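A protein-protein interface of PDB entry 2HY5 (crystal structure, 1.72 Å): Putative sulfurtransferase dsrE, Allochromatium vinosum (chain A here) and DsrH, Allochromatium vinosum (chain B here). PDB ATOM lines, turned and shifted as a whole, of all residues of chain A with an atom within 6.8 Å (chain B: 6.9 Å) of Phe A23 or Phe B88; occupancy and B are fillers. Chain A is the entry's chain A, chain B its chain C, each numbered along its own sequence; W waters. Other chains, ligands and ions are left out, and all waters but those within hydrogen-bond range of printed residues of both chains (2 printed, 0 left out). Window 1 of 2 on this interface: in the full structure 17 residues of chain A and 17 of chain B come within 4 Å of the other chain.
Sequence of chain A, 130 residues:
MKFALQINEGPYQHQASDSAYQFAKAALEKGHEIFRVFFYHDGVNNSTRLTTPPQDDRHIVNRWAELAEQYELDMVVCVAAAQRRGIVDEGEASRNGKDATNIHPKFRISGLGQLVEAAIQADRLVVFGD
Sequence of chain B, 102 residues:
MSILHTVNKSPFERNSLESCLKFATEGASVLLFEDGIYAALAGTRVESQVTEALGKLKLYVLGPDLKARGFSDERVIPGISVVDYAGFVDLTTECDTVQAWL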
ATOM      1  N   PHE A   3      -7.048 -12.341   6.002  1.00  0.00           N
ATOM      2  CA  PHE A   3      -5.716 -12.543   5.430  1.00  0.00           C
ATOM      3  C   PHE A   3      -4.819 -13.458   6.242  1.00  0.00           C
ATOM      4  O   PHE A   3      -4.890 -13.495   7.467  1.00  0.00           O
ATOM      5  CB  PHE A   3      -4.971 -11.211   5.325  1.00  0.00           C
ATOM      6  CG  PHE A   3      -5.457 -10.317   4.233  1.00  0.00           C
ATOM      7  CD1 PHE A   3      -5.041 -10.515   2.920  1.00  0.00           C
ATOM      8  CD2 PHE A   3      -6.325  -9.268   4.515  1.00  0.00           C
ATOM      9  CE1 PHE A   3      -5.487  -9.677   1.897  1.00  0.00           C
ATOM     10  CE2 PHE A   3      -6.775  -8.426   3.503  1.00  0.00           C
ATOM     11  CZ  PHE A   3      -6.357  -8.630   2.193  1.00  0.00           C
ATOM     12  N   LEU A   5      -0.791 -13.958   6.429  1.00  0.00           N
ATOM     13  CA  LEU A   5       0.455 -13.364   5.947  1.00  0.00           C
ATOM     14  C   LEU A   5       1.640 -14.252   6.295  1.00  0.00           C
ATOM     15  O   LEU A   5       1.754 -14.732   7.417  1.00  0.00           O
ATOM     16  CB  LEU A   5       0.669 -11.977   6.561  1.00  0.00           C
ATOM     17  CG  LEU A   5      -0.444 -10.945   6.362  1.00  0.00           C
ATOM     18  CD1 LEU A   5       0.007  -9.610   6.935  1.00  0.00           C
ATOM     19  CD2 LEU A   5      -0.782 -10.800   4.886  1.00  0.00           C
ATOM     20  N   ASP A  18       9.381  -5.482   6.494  1.00  0.00           N
ATOM     21  CA  ASP A  18       8.854  -4.117   6.490  1.00  0.00           C
ATOM     22  C   ASP A  18       7.644  -4.011   5.564  1.00  0.00           C
ATOM     23  O   ASP A  18       6.643  -3.376   5.894  1.00  0.00           O
ATOM     24  CB  ASP A  18       9.926  -3.132   6.021  1.00  0.00           C
ATOM     25  CG  ASP A  18      10.988  -2.885   7.069  1.00  0.00           C
ATOM     26  OD1 ASP A  18      10.709  -2.157   8.047  1.00  0.00           O
ATOM     27  OD2 ASP A  18      12.099  -3.434   6.913  1.00  0.00           O
ATOM     28  N   SER A  19       7.751  -4.628   4.396  1.00  0.00           N
ATOM     29  CA  SER A  19       6.653  -4.592   3.438  1.00  0.00           C
ATOM     30  C   SER A  19       5.429  -5.284   4.027  1.00  0.00           C
ATOM     31  O   SER A  19       4.301  -4.809   3.872  1.00  0.00           O
ATOM     32  CB  SER A  19       7.063  -5.279   2.137  1.00  0.00           C
ATOM     33  OG  SER A  19       8.123  -4.574   1.520  1.00  0.00           O
ATOM     34  N   ALA A  20       5.660  -6.405   4.701  1.00  0.00           N
ATOM     35  CA  ALA A  20       4.576  -7.164   5.312  1.00  0.00           C
ATOM     36  C   ALA A  20       3.922  -6.333   6.406  1.00  0.00           C
ATOM     37  O   ALA A  20       2.702  -6.339   6.557  1.00  0.00           O
ATOM     38  CB  ALA A  20       5.111  -8.474   5.884  1.00  0.00           C
ATOM     39  N   TYR A  21       4.738  -5.621   7.173  1.00  0.00           N
ATOM     40  CA  TYR A  21       4.220  -4.776   8.242  1.00  0.00           C
ATOM     41  C   TYR A  21       3.325  -3.670   7.683  1.00  0.00           C
ATOM     42  O   TYR A  21       2.202  -3.460   8.159  1.00  0.00           O
ATOM     43  CB  TYR A  21       5.368  -4.144   9.029  1.00  0.00           C
ATOM     44  CG  TYR A  21       4.882  -3.094   9.997  1.00  0.00           C
ATOM     45  CD1 TYR A  21       4.314  -3.452  11.221  1.00  0.00           C
ATOM     46  CD2 TYR A  21       4.909  -1.746   9.650  1.00  0.00           C
ATOM     47  CE1 TYR A  21       3.782  -2.487  12.073  1.00  0.00           C
ATOM     48  CE2 TYR A  21       4.374  -0.778  10.487  1.00  0.00           C
ATOM     49  CZ  TYR A  21       3.813  -1.152  11.696  1.00  0.00           C
ATOM     50  OH  TYR A  21       3.289  -0.182  12.521  1.00  0.00           O
ATOM     51  N   GLN A  22       3.819  -2.958   6.672  1.00  0.00           N
ATOM     52  CA  GLN A  22       3.040  -1.873   6.078  1.00  0.00           C
ATOM     53  C   GLN A  22       1.755  -2.398   5.448  1.00  0.00           C
ATOM     54  O   GLN A  22       0.722  -1.737   5.501  1.00  0.00           O
ATOM     55  CB  GLN A  22       3.877  -1.113   5.037  1.00  0.00           C
ATOM     56  CG  GLN A  22       5.158  -0.491   5.602  1.00  0.00           C
ATOM     57  CD  GLN A  22       4.903   0.596   6.639  1.00  0.00           C
ATOM     58  OE1 GLN A  22       5.788   0.942   7.431  1.00  0.00           O
ATOM     59  NE2 GLN A  22       3.703   1.151   6.627  1.00  0.00           N
ATOM     60  N   PHE A  23       1.817  -3.585   4.855  1.00  0.00           N
ATOM     61  CA  PHE A  23       0.628  -4.189   4.247  1.00  0.00           C
ATOM     62  C   PHE A  23      -0.381  -4.525   5.344  1.00  0.00           C
ATOM     63  O   PHE A  23      -1.567  -4.220   5.229  1.00  0.00           O
ATOM     64  CB  PHE A  23       0.987  -5.477   3.504  1.00  0.00           C
ATOM     65  CG  PHE A  23      -0.186  -6.124   2.821  1.00  0.00           C
ATOM     66  CD1 PHE A  23      -0.511  -5.795   1.510  1.00  0.00           C
ATOM     67  CD2 PHE A  23      -0.985  -7.039   3.499  1.00  0.00           C
ATOM     68  CE1 PHE A  23      -1.615  -6.368   0.881  1.00  0.00           C
ATOM     69  CE2 PHE A  23      -2.094  -7.620   2.883  1.00  0.00           C
ATOM     70  CZ  PHE A  23      -2.411  -7.284   1.571  1.00  0.00           C
ATOM     71  N   ALA A  24       0.102  -5.165   6.404  1.00  0.00           N
ATOM     72  CA  ALA A  24      -0.752  -5.550   7.521  1.00  0.00           C
ATOM     73  C   ALA A  24      -1.429  -4.341   8.137  1.00  0.00           C
ATOM     74  O   ALA A  24      -2.639  -4.354   8.380  1.00  0.00           O
ATOM     75  CB  ALA A  24       0.062  -6.274   8.583  1.00  0.00           C
ATOM     76  N   LYS A  25      -0.646  -3.304   8.406  1.00  0.00           N
ATOM     77  CA  LYS A  25      -1.191  -2.100   9.012  1.00  0.00           C
ATOM     78  C   LYS A  25      -2.272  -1.496   8.130  1.00  0.00           C
ATOM     79  O   LYS A  25      -3.336  -1.107   8.609  1.00  0.00           O
ATOM     80  CB  LYS A  25      -0.079  -1.078   9.256  1.00  0.00           C
ATOM     81  CG  LYS A  25      -0.488   0.045  10.202  1.00  0.00           C
ATOM     82  CD  LYS A  25       0.725   0.801  10.724  1.00  0.00           C
ATOM     83  CE  LYS A  25       1.223   1.822   9.725  1.00  0.00           C
ATOM     84  NZ  LYS A  25       0.283   2.975   9.627  1.00  0.00           N
ATOM     85  N   ALA A  26      -2.006  -1.431   6.830  1.00  0.00           N
ATOM     86  CA  ALA A  26      -2.976  -0.856   5.908  1.00  0.00           C
ATOM     87  C   ALA A  26      -4.249  -1.694   5.831  1.00  0.00           C
ATOM     88  O   ALA A  26      -5.355  -1.154   5.747  1.00  0.00           O
ATOM     89  CB  ALA A  26      -2.355  -0.713   4.519  1.00  0.00           C
ATOM     90  N   ALA A  27      -4.090  -3.013   5.862  1.00  0.00           N
ATOM     91  CA  ALA A  27      -5.225  -3.922   5.791  1.00  0.00           C
ATOM     92  C   ALA A  27      -6.057  -3.812   7.063  1.00  0.00           C
ATOM     93  O   ALA A  27      -7.285  -3.790   7.010  1.00  0.00           O
ATOM     94  CB  ALA A  27      -4.733  -5.343   5.612  1.00  0.00           C
ATOM     95  N   LEU A  28      -5.377  -3.742   8.202  1.00  0.00           N
ATOM     96  CA  LEU A  28      -6.055  -3.640   9.488  1.00  0.00           C
ATOM     97  C   LEU A  28      -6.821  -2.336   9.636  1.00  0.00           C
ATOM     98  O   LEU A  28      -7.904  -2.312  10.226  1.00  0.00           O
ATOM     99  CB  LEU A  28      -5.039  -3.795  10.622  1.00  0.00           C
ATOM    100  CG  LEU A  28      -4.499  -5.222  10.734  1.00  0.00           C
ATOM    101  CD1 LEU A  28      -3.254  -5.242  11.595  1.00  0.00           C
ATOM    102  CD2 LEU A  28      -5.574  -6.126  11.305  1.00  0.00           C
ATOM    103  N   GLU A  29      -6.274  -1.253   9.093  1.00  0.00           N
ATOM    104  CA  GLU A  29      -6.943   0.043   9.183  1.00  0.00           C
ATOM    105  C   GLU A  29      -8.185   0.075   8.296  1.00  0.00           C
ATOM    106  O   GLU A  29      -9.077   0.902   8.496  1.00  0.00           O
ATOM    107  CB  GLU A  29      -5.979   1.170   8.801  1.00  0.00           C
ATOM    108  CG  GLU A  29      -4.742   1.198   9.682  1.00  0.00           C
ATOM    109  CD  GLU A  29      -3.876   2.427   9.485  1.00  0.00           C
ATOM    110  OE1 GLU A  29      -3.802   2.948   8.350  1.00  0.00           O
ATOM    111  OE2 GLU A  29      -3.242   2.859  10.470  1.00  0.00           O
ATOM    112  N   LYS A  30      -8.238  -0.836   7.327  1.00  0.00           N
ATOM    113  CA  LYS A  30      -9.376  -0.943   6.414  1.00  0.00           C
ATOM    114  C   LYS A  30     -10.470  -1.835   6.994  1.00  0.00           C
ATOM    115  O   LYS A  30     -11.539  -1.980   6.402  1.00  0.00           O
ATOM    116  CB  LYS A  30      -8.931  -1.520   5.071  1.00  0.00           C
ATOM    117  CG  LYS A  30      -8.377  -0.502   4.093  1.00  0.00           C
ATOM    118  CD  LYS A  30      -7.867  -1.205   2.845  1.00  0.00           C
ATOM    119  CE  LYS A  30      -7.644  -0.236   1.708  1.00  0.00           C
ATOM    120  NZ  LYS A  30      -8.926   0.357   1.245  1.00  0.00           N
ATOM    121  N   ILE A  34      -6.706 -10.080   9.953  1.00  0.00           N
ATOM    122  CA  ILE A  34      -5.462 -10.780   9.674  1.00  0.00           C
ATOM    123  C   ILE A  34      -5.570 -11.978  10.608  1.00  0.00           C
ATOM    124  O   ILE A  34      -5.394 -11.859  11.822  1.00  0.00           O
ATOM    125  CB  ILE A  34      -4.221  -9.927  10.011  1.00  0.00           C
ATOM    126  CG1 ILE A  34      -4.109  -8.777   9.004  1.00  0.00           C
ATOM    127  CG2 ILE A  34      -2.956 -10.791   9.966  1.00  0.00           C
ATOM    128  CD1 ILE A  34      -2.901  -7.888   9.199  1.00  0.00           C
ATOM    129  N   VAL A 126      -0.941 -13.921   1.503  1.00  0.00           N
ATOM    130  CA  VAL A 126       0.017 -12.980   0.944  1.00  0.00           C
ATOM    131  C   VAL A 126       1.392 -13.290   1.513  1.00  0.00           C
ATOM    132  O   VAL A 126       1.613 -13.185   2.721  1.00  0.00           O
ATOM    133  CB  VAL A 126      -0.387 -11.530   1.274  1.00  0.00           C
ATOM    134  CG1 VAL A 126       0.481 -10.555   0.497  1.00  0.00           C
ATOM    135  CG2 VAL A 126      -1.851 -11.318   0.929  1.00  0.00           C
ATOM    136  N   PHE A 128       5.537 -12.707   1.690  1.00  0.00           N
ATOM    137  CA  PHE A 128       6.572 -11.696   1.552  1.00  0.00           C
ATOM    138  C   PHE A 128       7.918 -12.370   1.723  1.00  0.00           C
ATOM    139  O   PHE A 128       8.193 -12.967   2.761  1.00  0.00           O
ATOM    140  CB  PHE A 128       6.397 -10.603   2.611  1.00  0.00           C
ATOM    141  CG  PHE A 128       5.142  -9.791   2.441  1.00  0.00           C
ATOM    142  CD1 PHE A 128       3.921 -10.256   2.928  1.00  0.00           C
ATOM    143  CD2 PHE A 128       5.174  -8.579   1.758  1.00  0.00           C
ATOM    144  CE1 PHE A 128       2.746  -9.525   2.735  1.00  0.00           C
ATOM    145  CE2 PHE A 128       4.000  -7.835   1.557  1.00  0.00           C
ATOM    146  CZ  PHE A 128       2.787  -8.312   2.047  1.00  0.00           C
ATOM    147  N   LEU B   4      -3.491 -11.760  -8.819  1.00  0.00           N
ATOM    148  CA  LEU B   4      -2.674 -10.579  -8.612  1.00  0.00           C
ATOM    149  C   LEU B   4      -1.277 -11.142  -8.419  1.00  0.00           C
ATOM    150  O   LEU B   4      -1.019 -11.859  -7.449  1.00  0.00           O
ATOM    151  CB  LEU B   4      -3.062  -9.803  -7.350  1.00  0.00           C
ATOM    152  CG  LEU B   4      -1.987  -8.775  -6.960  1.00  0.00           C
ATOM    153  CD1 LEU B   4      -1.943  -7.655  -7.990  1.00  0.00           C
ATOM    154  CD2 LEU B   4      -2.255  -8.222  -5.568  1.00  0.00           C
ATOM    155  N   THR B   6       2.675 -10.580  -7.658  1.00  0.00           N
ATOM    156  CA  THR B   6       3.513  -9.578  -7.013  1.00  0.00           C
ATOM    157  C   THR B   6       4.963  -9.855  -7.391  1.00  0.00           C
ATOM    158  O   THR B   6       5.407 -11.004  -7.394  1.00  0.00           O
ATOM    159  CB  THR B   6       3.371  -9.596  -5.471  1.00  0.00           C
ATOM    160  OG1 THR B   6       3.772 -10.872  -4.958  1.00  0.00           O
ATOM    161  CG2 THR B   6       1.925  -9.313  -5.064  1.00  0.00           C
ATOM    162  N   LEU B  31       1.692  -6.327  -9.594  1.00  0.00           N
ATOM    163  CA  LEU B  31       2.120  -5.237  -8.735  1.00  0.00           C
ATOM    164  C   LEU B  31       3.613  -5.310  -8.517  1.00  0.00           C
ATOM    165  O   LEU B  31       4.148  -6.346  -8.105  1.00  0.00           O
ATOM    166  CB  LEU B  31       1.428  -5.284  -7.370  1.00  0.00           C
ATOM    167  CG  LEU B  31       2.002  -4.258  -6.379  1.00  0.00           C
ATOM    168  CD1 LEU B  31       1.628  -2.843  -6.819  1.00  0.00           C
ATOM    169  CD2 LEU B  31       1.480  -4.529  -4.986  1.00  0.00           C
ATOM    170  N   PHE B  33       6.686  -3.955  -6.395  1.00  0.00           N
ATOM    171  CA  PHE B  33       6.989  -3.271  -5.149  1.00  0.00           C
ATOM    172  C   PHE B  33       8.419  -3.601  -4.737  1.00  0.00           C
ATOM    173  O   PHE B  33       9.053  -4.461  -5.344  1.00  0.00           O
ATOM    174  CB  PHE B  33       5.946  -3.584  -4.055  1.00  0.00           C
ATOM    175  CG  PHE B  33       5.998  -4.985  -3.504  1.00  0.00           C
ATOM    176  CD1 PHE B  33       5.779  -6.090  -4.320  1.00  0.00           C
ATOM    177  CD2 PHE B  33       6.202  -5.192  -2.142  1.00  0.00           C
ATOM    178  CE1 PHE B  33       5.759  -7.379  -3.788  1.00  0.00           C
ATOM    179  CE2 PHE B  33       6.183  -6.475  -1.602  1.00  0.00           C
ATOM    180  CZ  PHE B  33       5.961  -7.570  -2.425  1.00  0.00           C
ATOM    181  N   LEU B  62       4.118   0.271  -6.597  1.00  0.00           N
ATOM    182  CA  LEU B  62       3.929   0.830  -5.261  1.00  0.00           C
ATOM    183  C   LEU B  62       4.647   2.170  -5.105  1.00  0.00           C
ATOM    184  O   LEU B  62       5.876   2.236  -5.088  1.00  0.00           O
ATOM    185  CB  LEU B  62       4.412  -0.172  -4.202  1.00  0.00           C
ATOM    186  CG  LEU B  62       4.057   0.155  -2.750  1.00  0.00           C
ATOM    187  CD1 LEU B  62       2.543   0.169  -2.552  1.00  0.00           C
ATOM    188  CD2 LEU B  62       4.693  -0.886  -1.849  1.00  0.00           C
ATOM    189  N   VAL B  83       0.070   3.047  -6.902  1.00  0.00           N
ATOM    190  CA  VAL B  83      -0.792   2.818  -5.746  1.00  0.00           C
ATOM    191  C   VAL B  83       0.007   2.896  -4.442  1.00  0.00           C
ATOM    192  O   VAL B  83       1.233   2.807  -4.452  1.00  0.00           O
ATOM    193  CB  VAL B  83      -1.448   1.425  -5.813  1.00  0.00           C
ATOM    194  CG1 VAL B  83      -2.272   1.296  -7.087  1.00  0.00           C
ATOM    195  CG2 VAL B  83      -0.372   0.343  -5.762  1.00  0.00           C
ATOM    196  N   ASP B  84      -0.685   3.088  -3.321  1.00  0.00           N
ATOM    197  CA  ASP B  84      -0.001   3.120  -2.032  1.00  0.00           C
ATOM    198  C   ASP B  84      -0.299   1.791  -1.354  1.00  0.00           C
ATOM    199  O   ASP B  84      -0.874   0.901  -1.973  1.00  0.00           O
ATOM    200  CB  ASP B  84      -0.478   4.288  -1.161  1.00  0.00           C
ATOM    201  CG  ASP B  84      -1.981   4.374  -1.069  1.00  0.00           C
ATOM    202  OD1 ASP B  84      -2.656   3.345  -1.275  1.00  0.00           O
ATOM    203  OD2 ASP B  84      -2.488   5.477  -0.777  1.00  0.00           O
ATOM    204  N   TYR B  85       0.086   1.638  -0.094  1.00  0.00           N
ATOM    205  CA  TYR B  85      -0.172   0.366   0.573  1.00  0.00           C
ATOM    206  C   TYR B  85      -1.658   0.036   0.666  1.00  0.00           C
ATOM    207  O   TYR B  85      -2.045  -1.130   0.568  1.00  0.00           O
ATOM    208  CB  TYR B  85       0.478   0.345   1.957  1.00  0.00           C
ATOM    209  CG  TYR B  85       1.972   0.077   1.901  1.00  0.00           C
ATOM    210  CD1 TYR B  85       2.898   1.093   2.147  1.00  0.00           C
ATOM    211  CD2 TYR B  85       2.456  -1.190   1.584  1.00  0.00           C
ATOM    212  CE1 TYR B  85       4.274   0.849   2.080  1.00  0.00           C
ATOM    213  CE2 TYR B  85       3.826  -1.446   1.514  1.00  0.00           C
ATOM    214  CZ  TYR B  85       4.727  -0.425   1.762  1.00  0.00           C
ATOM    215  OH  TYR B  85       6.080  -0.672   1.698  1.00  0.00           O
ATOM    216  N   ALA B  86      -2.496   1.055   0.844  1.00  0.00           N
ATOM    217  CA  ALA B  86      -3.931   0.816   0.913  1.00  0.00           C
ATOM    218  C   ALA B  86      -4.392   0.275  -0.443  1.00  0.00           C
ATOM    219  O   ALA B  86      -5.246  -0.603  -0.506  1.00  0.00           O
ATOM    220  CB  ALA B  86      -4.671   2.113   1.255  1.00  0.00           C
ATOM    221  N   GLY B  87      -3.810   0.798  -1.523  1.00  0.00           N
ATOM    222  CA  GLY B  87      -4.159   0.334  -2.855  1.00  0.00           C
ATOM    223  C   GLY B  87      -3.700  -1.097  -3.078  1.00  0.00           C
ATOM    224  O   GLY B  87      -4.355  -1.873  -3.773  1.00  0.00           O
ATOM    225  N   PHE B  88      -2.558  -1.433  -2.484  1.00  0.00           N
ATOM    226  CA  PHE B  88      -1.968  -2.767  -2.564  1.00  0.00           C
ATOM    227  C   PHE B  88      -2.975  -3.730  -1.933  1.00  0.00           C
ATOM    228  O   PHE B  88      -3.301  -4.777  -2.493  1.00  0.00           O
ATOM    229  CB  PHE B  88      -0.637  -2.741  -1.792  1.00  0.00           C
ATOM    230  CG  PHE B  88       0.180  -4.014  -1.861  1.00  0.00           C
ATOM    231  CD1 PHE B  88       1.484  -4.014  -1.377  1.00  0.00           C
ATOM    232  CD2 PHE B  88      -0.349  -5.208  -2.350  1.00  0.00           C
ATOM    233  CE1 PHE B  88       2.251  -5.179  -1.373  1.00  0.00           C
ATOM    234  CE2 PHE B  88       0.408  -6.377  -2.350  1.00  0.00           C
ATOM    235  CZ  PHE B  88       1.712  -6.363  -1.859  1.00  0.00           C
ATOM    236  N   VAL B  89      -3.480  -3.357  -0.764  1.00  0.00           N
ATOM    237  CA  VAL B  89      -4.466  -4.181  -0.077  1.00  0.00           C
ATOM    238  C   VAL B  89      -5.724  -4.362  -0.935  1.00  0.00           C
ATOM    239  O   VAL B  89      -6.239  -5.472  -1.049  1.00  0.00           O
ATOM    240  CB  VAL B  89      -4.866  -3.561   1.277  1.00  0.00           C
ATOM    241  CG1 VAL B  89      -6.062  -4.310   1.867  1.00  0.00           C
ATOM    242  CG2 VAL B  89      -3.690  -3.625   2.232  1.00  0.00           C
ATOM    243  N   ASP B  90      -6.224  -3.282  -1.531  1.00  0.00           N
ATOM    244  CA  ASP B  90      -7.419  -3.392  -2.366  1.00  0.00           C
ATOM    245  C   ASP B  90      -7.194  -4.322  -3.555  1.00  0.00           C
ATOM    246  O   ASP B  90      -8.110  -5.023  -3.977  1.00  0.00           O
ATOM    247  CB  ASP B  90      -7.871  -2.018  -2.870  1.00  0.00           C
ATOM    248  CG  ASP B  90      -8.497  -1.174  -1.780  1.00  0.00           C
ATOM    249  OD1 ASP B  90      -9.084  -1.749  -0.840  1.00  0.00           O
ATOM    250  OD2 ASP B  90      -8.417   0.068  -1.870  1.00  0.00           O
ATOM    251  N   LEU B  91      -5.983  -4.321  -4.103  1.00  0.00           N
ATOM    252  CA  LEU B  91      -5.685  -5.199  -5.226  1.00  0.00           C
ATOM    253  C   LEU B  91      -5.784  -6.669  -4.822  1.00  0.00           C
ATOM    254  O   LEU B  91      -6.272  -7.496  -5.592  1.00  0.00           O
ATOM    255  CB  LEU B  91      -4.286  -4.915  -5.785  1.00  0.00           C
ATOM    256  CG  LEU B  91      -4.130  -3.653  -6.640  1.00  0.00           C
ATOM    257  CD1 LEU B  91      -2.667  -3.465  -7.019  1.00  0.00           C
ATOM    258  CD2 LEU B  91      -4.996  -3.769  -7.888  1.00  0.00           C
ATOM    259  N   THR B  92      -5.325  -7.003  -3.618  1.00  0.00           N
ATOM    260  CA  THR B  92      -5.379  -8.395  -3.174  1.00  0.00           C
ATOM    261  C   THR B  92      -6.807  -8.872  -2.941  1.00  0.00           C
ATOM    262  O   THR B  92      -7.092 -10.062  -3.087  1.00  0.00           O
ATOM    263  CB  THR B  92      -4.579  -8.628  -1.868  1.00  0.00           C
ATOM    264  OG1 THR B  92      -5.176  -7.883  -0.799  1.00  0.00           O
ATOM    265  CG2 THR B  92      -3.126  -8.202  -2.048  1.00  0.00           C
ATOM    266  N   THR B  93      -7.705  -7.956  -2.577  1.00  0.00           N
ATOM    267  CA  THR B  93      -9.095  -8.335  -2.338  1.00  0.00           C
ATOM    268  C   THR B  93      -9.939  -8.282  -3.609  1.00  0.00           C
ATOM    269  O   THR B  93     -10.920  -9.018  -3.738  1.00  0.00           O
ATOM    270  CB  THR B  93      -9.760  -7.451  -1.252  1.00  0.00           C
ATOM    271  OG1 THR B  93      -9.740  -6.077  -1.653  1.00  0.00           O
ATOM    272  CG2 THR B  93      -9.024  -7.595   0.067  1.00  0.00           C
ATOM    273  N   VAL B  98      -3.553 -14.248  -4.809  1.00  0.00           N
ATOM    274  CA  VAL B  98      -2.310 -13.498  -4.888  1.00  0.00           C
ATOM    275  C   VAL B  98      -1.189 -14.502  -5.111  1.00  0.00           C
ATOM    276  O   VAL B  98      -1.144 -15.547  -4.465  1.00  0.00           O
ATOM    277  CB  VAL B  98      -2.028 -12.720  -3.587  1.00  0.00           C
ATOM    278  CG1 VAL B  98      -0.767 -11.871  -3.753  1.00  0.00           C
ATOM    279  CG2 VAL B  98      -3.221 -11.840  -3.230  1.00  0.00           C
HETATM  280  O   HOH W   1       6.966  -2.499   0.172  1.00  0.00           O
HETATM  281  O   HOH W   2     -10.876   1.051  -1.533  1.00  0.00           O
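The side-chain amino group (NZ) of Lys A30 lies within salt-bridge range of the side-chain carboxylate (OD1) of Asp B90, 3.0 Å away.
OG1 of Thr B92 touches CE1 of Phe A3, 3.3 Å away.
CZ of Tyr B85 touches CB of Gln A22, at 3.5 Å.
Phe A23 touches Phe B88.
Phe A23 touches Val B89 (CE1 to CG2, 3.7 Å).
Thr B92 touches Phe A23 (OG1 to CZ, 3.7 Å).
CB of Ala A26 touches CB of Tyr B85, 3.96 Å away.
CB of Ala A26 touches CG2 of Val B89, at 3.9 Å.
Ala A27 touches Val B89 (N to CG2, 3.7 Å).
Ala B86 touches Lys A30.
Lys A30 touches Val B89 (CD to CG1, 3.7 Å).
The backbone NH (N) of Ala B86 lies within hydrogen-bond range of the side-chain carboxylate (OD1) of Asp B84, at 3.1 Å.
The side-chain hydroxyl (OG1) of Thr B92 sits at hydrogen-bond distance from the backbone carbonyl oxygen (O) of Val B89, at 2.6 Å.
The backbone carbonyl oxygen (O) of Asp B90 sits at hydrogen-bond distance from the side-chain hydroxyl (OG1) of Thr B93 (3.0 Å).
Water W1 lies within hydrogen-bond range of OH of Tyr B85 and OG of Ser A19.
Water W2 bridges the side-chain carboxylate (OD2) of Asp B90 and the side-chain amino group (NZ) of Lys A30.
Phe B88 touches just one residue of chain A: Phe A23.
Of the printed residues of chain A, Ala B86 touches Lys A30 (3.3 Å).
Of the printed residues of chain B, Lys A30 touches Ala B86, Val B89 and Asp B90.
Printed residues of chain A within 4 Å of Tyr B85: Gln A22 (3.5 Å) and Ala A26 (3.96 Å).
Printed residues of chain B within 4 Å of Phe A3: Thr B92 and Thr B93.
Phe B33 touches none of the printed residues of chain A.
The nearest residue of chain A that does not touch Phe B88 is Phe A128 (4.3 Å).
The nearest printed residue of chain B that does not touch Ala A27 is Tyr B85 (6.0 Å).
Hydrophobic or aromatic side chains of chain A that line the printed part of chain B: Phe A3, Phe A23, Ala A26 and Ala A27.
Of the 17 printed residues of chain B, 7 touch a printed residue of chain A.
Among the printed residues, 12 pairs touch across the chains.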
